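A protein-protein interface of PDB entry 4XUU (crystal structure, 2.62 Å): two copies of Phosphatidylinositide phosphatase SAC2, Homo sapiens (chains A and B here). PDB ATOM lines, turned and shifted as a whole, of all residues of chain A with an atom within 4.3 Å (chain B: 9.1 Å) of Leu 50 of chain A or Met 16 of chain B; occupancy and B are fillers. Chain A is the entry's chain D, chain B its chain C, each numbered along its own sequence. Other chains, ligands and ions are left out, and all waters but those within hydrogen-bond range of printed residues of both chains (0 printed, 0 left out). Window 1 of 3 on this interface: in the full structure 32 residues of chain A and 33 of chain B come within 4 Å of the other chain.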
ATOM      1  N   LEU A  19       3.937  19.110  24.593  1.00  0.00           N
ATOM      2  CA  LEU A  19       2.786  19.396  23.737  1.00  0.00           C
ATOM      3  C   LEU A  19       2.332  20.850  23.775  1.00  0.00           C
ATOM      4  O   LEU A  19       2.058  21.455  22.736  1.00  0.00           O
ATOM      5  CB  LEU A  19       1.606  18.513  24.145  1.00  0.00           C
ATOM      6  CG  LEU A  19       1.294  17.264  23.326  1.00  0.00           C
ATOM      7  CD1 LEU A  19       2.427  16.247  23.395  1.00  0.00           C
ATOM      8  CD2 LEU A  19      -0.024  16.664  23.803  1.00  0.00           C
ATOM      9  N   TRP A  30     -10.337  14.875  23.093  1.00  0.00           N
ATOM     10  CA  TRP A  30     -11.305  13.923  22.537  1.00  0.00           C
ATOM     11  C   TRP A  30     -10.869  13.420  21.177  1.00  0.00           C
ATOM     12  O   TRP A  30     -10.331  14.179  20.361  1.00  0.00           O
ATOM     13  CB  TRP A  30     -12.702  14.555  22.413  1.00  0.00           C
ATOM     14  CG  TRP A  30     -13.162  15.187  23.673  1.00  0.00           C
ATOM     15  CD1 TRP A  30     -13.876  14.597  24.678  1.00  0.00           C
ATOM     16  CD2 TRP A  30     -12.908  16.532  24.091  1.00  0.00           C
ATOM     17  NE1 TRP A  30     -14.089  15.500  25.696  1.00  0.00           N
ATOM     18  CE2 TRP A  30     -13.504  16.694  25.360  1.00  0.00           C
ATOM     19  CE3 TRP A  30     -12.239  17.617  23.513  1.00  0.00           C
ATOM     20  CZ2 TRP A  30     -13.454  17.897  26.058  1.00  0.00           C
ATOM     21  CZ3 TRP A  30     -12.187  18.816  24.210  1.00  0.00           C
ATOM     22  CH2 TRP A  30     -12.792  18.945  25.469  1.00  0.00           C
ATOM     23  N   VAL A  49      -9.593  12.561  13.905  1.00  0.00           N
ATOM     24  CA  VAL A  49      -9.255  13.912  14.321  1.00  0.00           C
ATOM     25  C   VAL A  49      -9.067  13.940  15.829  1.00  0.00           C
ATOM     26  O   VAL A  49      -9.881  13.391  16.575  1.00  0.00           O
ATOM     27  CB  VAL A  49     -10.339  14.944  13.916  1.00  0.00           C
ATOM     28  CG1 VAL A  49      -9.933  16.344  14.363  1.00  0.00           C
ATOM     29  CG2 VAL A  49     -10.590  14.916  12.407  1.00  0.00           C
ATOM     30  N   LEU A  50      -7.982  14.567  16.269  1.00  0.00           N
ATOM     31  CA  LEU A  50      -7.755  14.793  17.687  1.00  0.00           C
ATOM     32  C   LEU A  50      -8.048  16.250  18.033  1.00  0.00           C
ATOM     33  O   LEU A  50      -7.465  17.164  17.444  1.00  0.00           O
ATOM     34  CB  LEU A  50      -6.323  14.424  18.065  1.00  0.00           C
ATOM     35  CG  LEU A  50      -5.931  14.424  19.545  1.00  0.00           C
ATOM     36  CD1 LEU A  50      -6.732  13.397  20.349  1.00  0.00           C
ATOM     37  CD2 LEU A  50      -4.435  14.169  19.672  1.00  0.00           C
ATOM     38  N   LEU A  51      -8.967  16.451  18.976  1.00  0.00           N
ATOM     39  CA  LEU A  51      -9.277  17.779  19.491  1.00  0.00           C
ATOM     40  C   LEU A  51      -8.780  17.898  20.931  1.00  0.00           C
ATOM     41  O   LEU A  51      -9.212  17.144  21.814  1.00  0.00           O
ATOM     42  CB  LEU A  51     -10.784  18.059  19.406  1.00  0.00           C
ATOM     43  CG  LEU A  51     -11.369  19.329  20.041  1.00  0.00           C
ATOM     44  CD1 LEU A  51     -10.892  20.604  19.333  1.00  0.00           C
ATOM     45  CD2 LEU A  51     -12.889  19.272  20.054  1.00  0.00           C
ATOM     46  N   LEU A  52      -7.860  18.832  21.156  1.00  0.00           N
ATOM     47  CA  LEU A  52      -7.315  19.075  22.487  1.00  0.00           C
ATOM     48  C   LEU A  52      -7.660  20.478  22.934  1.00  0.00           C
ATOM     49  O   LEU A  52      -7.658  21.398  22.129  1.00  0.00           O
ATOM     50  CB  LEU A  52      -5.792  18.907  22.491  1.00  0.00           C
ATOM     51  CG  LEU A  52      -5.194  17.535  22.185  1.00  0.00           C
ATOM     52  CD1 LEU A  52      -3.676  17.631  22.110  1.00  0.00           C
ATOM     53  CD2 LEU A  52      -5.619  16.491  23.212  1.00  0.00           C
ATOM     54  N   TYR A  59      -6.755  22.568  20.017  1.00  0.00           N
ATOM     55  CA  TYR A  59      -5.831  21.969  19.059  1.00  0.00           C
ATOM     56  C   TYR A  59      -6.562  20.946  18.215  1.00  0.00           C
ATOM     57  O   TYR A  59      -7.288  20.098  18.743  1.00  0.00           O
ATOM     58  CB  TYR A  59      -4.653  21.308  19.785  1.00  0.00           C
ATOM     59  CG  TYR A  59      -3.793  22.269  20.573  1.00  0.00           C
ATOM     60  CD1 TYR A  59      -4.229  22.791  21.794  1.00  0.00           C
ATOM     61  CD2 TYR A  59      -2.541  22.656  20.100  1.00  0.00           C
ATOM     62  CE1 TYR A  59      -3.444  23.677  22.518  1.00  0.00           C
ATOM     63  CE2 TYR A  59      -1.746  23.537  20.823  1.00  0.00           C
ATOM     64  CZ  TYR A  59      -2.207  24.046  22.028  1.00  0.00           C
ATOM     65  OH  TYR A  59      -1.429  24.924  22.741  1.00  0.00           O
ATOM     66  N   VAL A  60      -6.375  21.040  16.904  1.00  0.00           N
ATOM     67  CA  VAL A  60      -7.040  20.148  15.966  1.00  0.00           C
ATOM     68  C   VAL A  60      -5.984  19.490  15.089  1.00  0.00           C
ATOM     69  O   VAL A  60      -5.207  20.175  14.426  1.00  0.00           O
ATOM     70  CB  VAL A  60      -8.089  20.892  15.095  1.00  0.00           C
ATOM     71  CG1 VAL A  60      -8.847  19.912  14.212  1.00  0.00           C
ATOM     72  CG2 VAL A  60      -9.070  21.683  15.969  1.00  0.00           C
ATOM     73  N   ALA A  61      -5.957  18.159  15.110  1.00  0.00           N
ATOM     74  CA  ALA A  61      -4.974  17.387  14.364  1.00  0.00           C
ATOM     75  C   ALA A  61      -5.639  16.282  13.550  1.00  0.00           C
ATOM     76  O   ALA A  61      -6.394  15.468  14.086  1.00  0.00           O
ATOM     77  CB  ALA A  61      -3.935  16.804  15.306  1.00  0.00           C
ATOM     78  N   TYR A  63      -5.251  12.904  11.432  1.00  0.00           N
ATOM     79  CA  TYR A  63      -4.377  11.755  11.212  1.00  0.00           C
ATOM     80  C   TYR A  63      -4.509  11.230   9.785  1.00  0.00           C
ATOM     81  O   TYR A  63      -5.555  11.391   9.150  1.00  0.00           O
ATOM     82  CB  TYR A  63      -4.675  10.645  12.222  1.00  0.00           C
ATOM     83  CG  TYR A  63      -4.089  10.886  13.599  1.00  0.00           C
ATOM     84  CD1 TYR A  63      -4.731  11.712  14.520  1.00  0.00           C
ATOM     85  CD2 TYR A  63      -2.892  10.285  13.979  1.00  0.00           C
ATOM     86  CE1 TYR A  63      -4.194  11.933  15.788  1.00  0.00           C
ATOM     87  CE2 TYR A  63      -2.345  10.497  15.245  1.00  0.00           C
ATOM     88  CZ  TYR A  63      -3.001  11.323  16.143  1.00  0.00           C
ATOM     89  OH  TYR A  63      -2.459  11.532  17.395  1.00  0.00           O
ATOM     90  N   SER B   9       4.323  17.884  14.927  1.00  0.00           N
ATOM     91  CA  SER B   9       3.513  16.750  14.492  1.00  0.00           C
ATOM     92  C   SER B   9       4.129  15.405  14.892  1.00  0.00           C
ATOM     93  O   SER B   9       3.409  14.476  15.260  1.00  0.00           O
ATOM     94  CB  SER B   9       3.289  16.803  12.980  1.00  0.00           C
ATOM     95  OG  SER B   9       2.628  18.000  12.614  1.00  0.00           O
ATOM     96  N   GLN B  10       5.457  15.308  14.820  1.00  0.00           N
ATOM     97  CA  GLN B  10       6.159  14.088  15.209  1.00  0.00           C
ATOM     98  C   GLN B  10       6.108  13.849  16.708  1.00  0.00           C
ATOM     99  O   GLN B  10       5.983  12.707  17.149  1.00  0.00           O
ATOM    100  CB  GLN B  10       7.610  14.105  14.733  1.00  0.00           C
ATOM    101  CG  GLN B  10       7.796  13.593  13.315  1.00  0.00           C
ATOM    102  CD  GLN B  10       9.243  13.636  12.857  1.00  0.00           C
ATOM    103  OE1 GLN B  10       9.526  13.630  11.658  1.00  0.00           O
ATOM    104  NE2 GLN B  10      10.169  13.678  13.810  1.00  0.00           N
ATOM    105  N   LEU B  11       6.211  14.926  17.485  1.00  0.00           N
ATOM    106  CA  LEU B  11       6.089  14.841  18.939  1.00  0.00           C
ATOM    107  C   LEU B  11       4.723  14.325  19.346  1.00  0.00           C
ATOM    108  O   LEU B  11       4.621  13.434  20.186  1.00  0.00           O
ATOM    109  CB  LEU B  11       6.348  16.198  19.601  1.00  0.00           C
ATOM    110  CG  LEU B  11       7.725  16.417  20.230  1.00  0.00           C
ATOM    111  CD1 LEU B  11       7.852  17.845  20.698  1.00  0.00           C
ATOM    112  CD2 LEU B  11       7.972  15.456  21.394  1.00  0.00           C
ATOM    113  N   LEU B  12       3.684  14.887  18.734  1.00  0.00           N
ATOM    114  CA  LEU B  12       2.304  14.497  18.998  1.00  0.00           C
ATOM    115  C   LEU B  12       2.053  13.029  18.656  1.00  0.00           C
ATOM    116  O   LEU B  12       1.467  12.303  19.459  1.00  0.00           O
ATOM    117  CB  LEU B  12       1.338  15.408  18.237  1.00  0.00           C
ATOM    118  CG  LEU B  12      -0.131  15.415  18.675  1.00  0.00           C
ATOM    119  CD1 LEU B  12      -0.311  16.075  20.037  1.00  0.00           C
ATOM    120  CD2 LEU B  12      -0.971  16.120  17.634  1.00  0.00           C
ATOM    121  N   GLN B  13       2.506  12.603  17.473  1.00  0.00           N
ATOM    122  CA  GLN B  13       2.435  11.201  17.046  1.00  0.00           C
ATOM    123  C   GLN B  13       3.054  10.277  18.081  1.00  0.00           C
ATOM    124  O   GLN B  13       2.423   9.320  18.534  1.00  0.00           O
ATOM    125  CB  GLN B  13       3.198  10.998  15.740  1.00  0.00           C
ATOM    126  CG  GLN B  13       2.466  11.380  14.479  1.00  0.00           C
ATOM    127  CD  GLN B  13       3.396  11.446  13.278  1.00  0.00           C
ATOM    128  OE1 GLN B  13       3.138  12.182  12.327  1.00  0.00           O
ATOM    129  NE2 GLN B  13       4.489  10.683  13.321  1.00  0.00           N
ATOM    130  N   SER B  14       4.303  10.578  18.430  1.00  0.00           N
ATOM    131  CA  SER B  14       5.080   9.805  19.388  1.00  0.00           C
ATOM    132  C   SER B  14       4.382   9.718  20.740  1.00  0.00           C
ATOM    133  O   SER B  14       4.355   8.659  21.365  1.00  0.00           O
ATOM    134  CB  SER B  14       6.469  10.428  19.550  1.00  0.00           C
ATOM    135  OG  SER B  14       7.172   9.833  20.621  1.00  0.00           O
ATOM    136  N   TYR B  15       3.810  10.837  21.172  1.00  0.00           N
ATOM    137  CA  TYR B  15       3.136  10.919  22.458  1.00  0.00           C
ATOM    138  C   TYR B  15       1.886  10.055  22.570  1.00  0.00           C
ATOM    139  O   TYR B  15       1.692   9.373  23.573  1.00  0.00           O
ATOM    140  CB  TYR B  15       2.768  12.363  22.782  1.00  0.00           C
ATOM    141  CG  TYR B  15       2.062  12.509  24.107  1.00  0.00           C
ATOM    142  CD1 TYR B  15       2.545  11.873  25.250  1.00  0.00           C
ATOM    143  CD2 TYR B  15       0.893  13.251  24.215  1.00  0.00           C
ATOM    144  CE1 TYR B  15       1.906  11.997  26.463  1.00  0.00           C
ATOM    145  CE2 TYR B  15       0.242  13.383  25.430  1.00  0.00           C
ATOM    146  CZ  TYR B  15       0.756  12.753  26.549  1.00  0.00           C
ATOM    147  OH  TYR B  15       0.116  12.875  27.757  1.00  0.00           O
ATOM    148  N   MET B  16       1.032  10.100  21.554  1.00  0.00           N
ATOM    149  CA  MET B  16      -0.204   9.323  21.578  1.00  0.00           C
ATOM    150  C   MET B  16       0.074   7.824  21.441  1.00  0.00           C
ATOM    151  O   MET B  16      -0.722   6.997  21.889  1.00  0.00           O
ATOM    152  CB  MET B  16      -1.195   9.823  20.518  1.00  0.00           C
ATOM    153  CG  MET B  16      -1.644  11.277  20.720  1.00  0.00           C
ATOM    154  SD  MET B  16      -2.689  11.601  22.355  1.00  0.00           S
ATOM    155  CE  MET B  16      -2.319  13.498  22.600  1.00  0.00           C
ATOM    156  N   LYS B  17       1.212   7.484  20.840  1.00  0.00           N
ATOM    157  CA  LYS B  17       1.647   6.096  20.744  1.00  0.00           C
ATOM    158  C   LYS B  17       2.186   5.601  22.087  1.00  0.00           C
ATOM    159  O   LYS B  17       1.882   4.484  22.507  1.00  0.00           O
ATOM    160  CB  LYS B  17       2.707   5.938  19.652  1.00  0.00           C
ATOM    161  CG  LYS B  17       2.938   4.499  19.209  1.00  0.00           C
ATOM    162  CD  LYS B  17       4.111   4.392  18.238  1.00  0.00           C
ATOM    163  CE  LYS B  17       4.229   2.991  17.651  1.00  0.00           C
ATOM    164  NZ  LYS B  17       4.604   1.968  18.667  1.00  0.00           N
ATOM    165  N   LEU B  18       2.977   6.440  22.756  1.00  0.00           N
ATOM    166  CA  LEU B  18       3.612   6.080  24.028  1.00  0.00           C
ATOM    167  C   LEU B  18       2.619   6.060  25.190  1.00  0.00           C
ATOM    168  O   LEU B  18       2.782   5.292  26.140  1.00  0.00           O
ATOM    169  CB  LEU B  18       4.770   7.034  24.349  1.00  0.00           C
ATOM    170  CG  LEU B  18       6.108   6.863  23.617  1.00  0.00           C
ATOM    171  CD1 LEU B  18       6.893   8.168  23.622  1.00  0.00           C
ATOM    172  CD2 LEU B  18       6.941   5.737  24.219  1.00  0.00           C
ATOM    173  N   LEU B  19       1.592   6.901  25.097  1.00  0.00           N
ATOM    174  CA  LEU B  19       0.591   7.068  26.157  1.00  0.00           C
ATOM    175  C   LEU B  19      -0.172   5.785  26.502  1.00  0.00           C
ATOM    176  O   LEU B  19      -0.537   5.572  27.660  1.00  0.00           O
ATOM    177  CB  LEU B  19      -0.399   8.170  25.764  1.00  0.00           C
ATOM    178  CG  LEU B  19      -1.378   8.723  26.803  1.00  0.00           C
ATOM    179  CD1 LEU B  19      -0.680   9.669  27.769  1.00  0.00           C
ATOM    180  CD2 LEU B  19      -2.530   9.430  26.112  1.00  0.00           C
ATOM    181  N   LEU B  20      -0.405   4.941  25.497  1.00  0.00           N
ATOM    182  CA  LEU B  20      -1.215   3.731  25.655  1.00  0.00           C
ATOM    183  C   LEU B  20      -0.578   2.506  24.993  1.00  0.00           C
ATOM    184  O   LEU B  20       0.199   2.653  24.052  1.00  0.00           O
ATOM    185  CB  LEU B  20      -2.607   3.947  25.053  1.00  0.00           C
ATOM    186  CG  LEU B  20      -3.477   5.121  25.494  1.00  0.00           C
ATOM    187  CD1 LEU B  20      -4.735   5.156  24.645  1.00  0.00           C
ATOM    188  CD2 LEU B  20      -3.826   5.035  26.970  1.00  0.00           C
ATOM    189  N   PRO B  21      -0.919   1.290  25.472  1.00  0.00           N
ATOM    190  CA  PRO B  21      -0.490   0.043  24.827  1.00  0.00           C
ATOM    191  C   PRO B  21      -0.892  -0.047  23.351  1.00  0.00           C
ATOM    192  O   PRO B  21      -1.857   0.599  22.931  1.00  0.00           O
ATOM    193  CB  PRO B  21      -1.221  -1.032  25.634  1.00  0.00           C
ATOM    194  CG  PRO B  21      -1.397  -0.429  26.975  1.00  0.00           C
ATOM    195  CD  PRO B  21      -1.640   1.027  26.734  1.00  0.00           C
ATOM    196  N   ASP B  22      -0.153  -0.854  22.592  1.00  0.00           N
ATOM    197  CA  ASP B  22      -0.341  -1.025  21.143  1.00  0.00           C
ATOM    198  C   ASP B  22      -1.798  -1.164  20.686  1.00  0.00           C
ATOM    199  O   ASP B  22      -2.198  -0.557  19.691  1.00  0.00           O
ATOM    200  CB  ASP B  22       0.462  -2.237  20.641  1.00  0.00           C
ATOM    201  CG  ASP B  22       1.928  -1.913  20.373  1.00  0.00           C
ATOM    202  OD1 ASP B  22       2.247  -0.758  20.018  1.00  0.00           O
ATOM    203  OD2 ASP B  22       2.768  -2.830  20.503  1.00  0.00           O
ATOM    204  N   GLU B  24      -4.668  -0.285  22.102  1.00  0.00           N
ATOM    205  CA  GLU B  24      -5.632   0.650  22.680  1.00  0.00           C
ATOM    206  C   GLU B  24      -5.714   1.968  21.909  1.00  0.00           C
ATOM    207  O   GLU B  24      -4.696   2.501  21.459  1.00  0.00           O
ATOM    208  CB  GLU B  24      -5.319   0.910  24.156  1.00  0.00           C
ATOM    209  CG  GLU B  24      -5.667  -0.257  25.079  1.00  0.00           C
ATOM    210  CD  GLU B  24      -5.467   0.060  26.555  1.00  0.00           C
ATOM    211  OE1 GLU B  24      -5.630   1.234  26.959  1.00  0.00           O
ATOM    212  OE2 GLU B  24      -5.157  -0.873  27.322  1.00  0.00           O
ATOM    213  N   LYS B  25      -6.938   2.468  21.752  1.00  0.00           N
ATOM    214  CA  LYS B  25      -7.200   3.757  21.113  1.00  0.00           C
ATOM    215  C   LYS B  25      -7.640   4.754  22.168  1.00  0.00           C
ATOM    216  O   LYS B  25      -8.432   4.421  23.049  1.00  0.00           O
ATOM    217  CB  LYS B  25      -8.311   3.636  20.068  1.00  0.00           C
ATOM    218  CG  LYS B  25      -8.017   2.696  18.911  1.00  0.00           C
ATOM    219  CD  LYS B  25      -7.494   3.435  17.686  1.00  0.00           C
ATOM    220  CE  LYS B  25      -7.330   2.473  16.518  1.00  0.00           C
ATOM    221  NZ  LYS B  25      -7.048   3.184  15.240  1.00  0.00           N
ATOM    222  N   PHE B  26      -7.123   5.975  22.066  1.00  0.00           N
ATOM    223  CA  PHE B  26      -7.543   7.088  22.900  1.00  0.00           C
ATOM    224  C   PHE B  26      -8.961   7.501  22.515  1.00  0.00           C
ATOM    225  O   PHE B  26      -9.266   7.665  21.337  1.00  0.00           O
ATOM    226  CB  PHE B  26      -6.567   8.253  22.703  1.00  0.00           C
ATOM    227  CG  PHE B  26      -6.918   9.495  23.474  1.00  0.00           C
ATOM    228  CD1 PHE B  26      -6.589   9.612  24.824  1.00  0.00           C
ATOM    229  CD2 PHE B  26      -7.551  10.566  22.841  1.00  0.00           C
ATOM    230  CE1 PHE B  26      -6.904  10.777  25.534  1.00  0.00           C
ATOM    231  CE2 PHE B  26      -7.869  11.732  23.540  1.00  0.00           C
ATOM    232  CZ  PHE B  26      -7.545  11.838  24.886  1.00  0.00           C
ATOM    233  N   HIS B  27      -9.825   7.646  23.515  1.00  0.00           N
ATOM    234  CA  HIS B  27     -11.185   8.140  23.304  1.00  0.00           C
ATOM    235  C   HIS B  27     -11.374   9.527  23.921  1.00  0.00           C
ATOM    236  O   HIS B  27     -12.005  10.402  23.327  1.00  0.00           O
ATOM    237  CB  HIS B  27     -12.208   7.165  23.892  1.00  0.00           C
ATOM    238  CG  HIS B  27     -12.533   6.007  23.000  1.00  0.00           C
ATOM    239  ND1 HIS B  27     -11.634   5.480  22.097  1.00  0.00           N
ATOM    240  CD2 HIS B  27     -13.653   5.256  22.893  1.00  0.00           C
ATOM    241  CE1 HIS B  27     -12.194   4.466  21.461  1.00  0.00           C
ATOM    242  NE2 HIS B  27     -13.419   4.309  21.927  1.00  0.00           N
ATOM    243  N   GLY B  28     -10.821   9.723  25.113  1.00  0.00           N
ATOM    244  CA  GLY B  28     -11.020  10.969  25.833  1.00  0.00           C
ATOM    245  C   GLY B  28     -10.075  11.152  26.993  1.00  0.00           C
ATOM    246  O   GLY B  28      -9.475  10.191  27.473  1.00  0.00           O
ATOM    247  N   GLY B  29      -9.946  12.398  27.434  1.00  0.00           N
ATOM    248  CA  GLY B  29      -9.051  12.748  28.531  1.00  0.00           C
ATOM    249  C   GLY B  29      -9.451  14.066  29.144  1.00  0.00           C
ATOM    250  O   GLY B  29      -9.841  14.993  28.430  1.00  0.00           O
ATOM    251  N   LEU B  52      -7.804   9.490  31.917  1.00  0.00           N
ATOM    252  CA  LEU B  52      -7.718   9.157  30.496  1.00  0.00           C
ATOM    253  C   LEU B  52      -8.556   7.930  30.164  1.00  0.00           C
ATOM    254  O   LEU B  52      -8.633   6.990  30.949  1.00  0.00           O
ATOM    255  CB  LEU B  52      -6.260   8.926  30.080  1.00  0.00           C
ATOM    256  CG  LEU B  52      -5.267  10.061  30.339  1.00  0.00           C
ATOM    257  CD1 LEU B  52      -3.834   9.603  30.089  1.00  0.00           C
ATOM    258  CD2 LEU B  52      -5.600  11.294  29.508  1.00  0.00           C
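CD2 of Leu 19 of chain A touches CD1 of Leu 12 of chain B, 3.8 Å away. Leu 19 of chain A touches Tyr 15 of chain B. Trp 30 of chain A touches His 27 of chain B. Met 16 of chain B touches Leu 50 of chain A. Phe 26 of chain B touches Leu 50 of chain A (CE2 to CD1, 3.8 Å). CD2 of Leu 12 of chain B touches CB of Ala 61 of chain A, at 3.8 Å. OH of Tyr 63 of chain A touches CG of Met 16 of chain B (3.4 Å).
Of the printed residues of chain B, Trp 30 of chain A touches His 27 (3.7 Å). No residue of chain B comes within 4 Å of Val 49 of chain A. Leu 50 of chain A touches just these residues of chain B: Met 16 (3.7 Å) and Phe 26 (3.8 Å). Ala 61 of chain A touches just one residue of chain B: Leu 12 (3.8 Å). Printed residues of chain B within 4 Å of Tyr 63 of chain A: Met 16 (3.4 Å). Printed residues of chain A within 4 Å of Leu 12 of chain B: Leu 19 (3.8 Å) and Ala 61 (3.8 Å). Of the printed residues of chain A, Met 16 of chain B touches Leu 50 and Tyr 63. Printed residues of chain A within 4 Å of Phe 26 of chain B: Leu 50 (3.8 Å). The nearest residue of chain B that does not touch Leu 50 of chain A is Leu 12 of chain B (4.5 Å). The nearest printed residue of chain A that does not touch Phe 26 of chain B is Trp 30 of chain A (4.02 Å).
The backbone carbonyl oxygen (O) of Leu 51 of chain A sits at hydrogen-bond distance from the backbone NH (N) of Trp 30 of chain A (2.8 Å). N of Leu 50 of chain A lies within hydrogen-bond range of O of Ala 61 of chain A, 2.8 Å away.
Hydrophobic or aromatic side chains of chain A that line the printed part of chain B: Leu 19, Leu 50, Ala 61 and Tyr 63. Along chain A the printed residues that touch a printed residue of chain B span positions 19 to 63. Printed residues of chain B that touch a printed residue of chain A: Leu 12, Tyr 15, Met 16, Phe 26 and His 27. Hydrophobic or aromatic side chains of chain B that line the printed part of chain A: Leu 12, Tyr 15, Met 16 and Phe 26. Along chain B the printed residues that touch a printed residue of chain A span positions 12 to 27. Among the printed residues, 7 pairs touch across the chains.
2 positions are printed for both chains. Of the 7 pairs that touch across the chains among the printed residues, none has its exchanged pair printed and touching as well.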
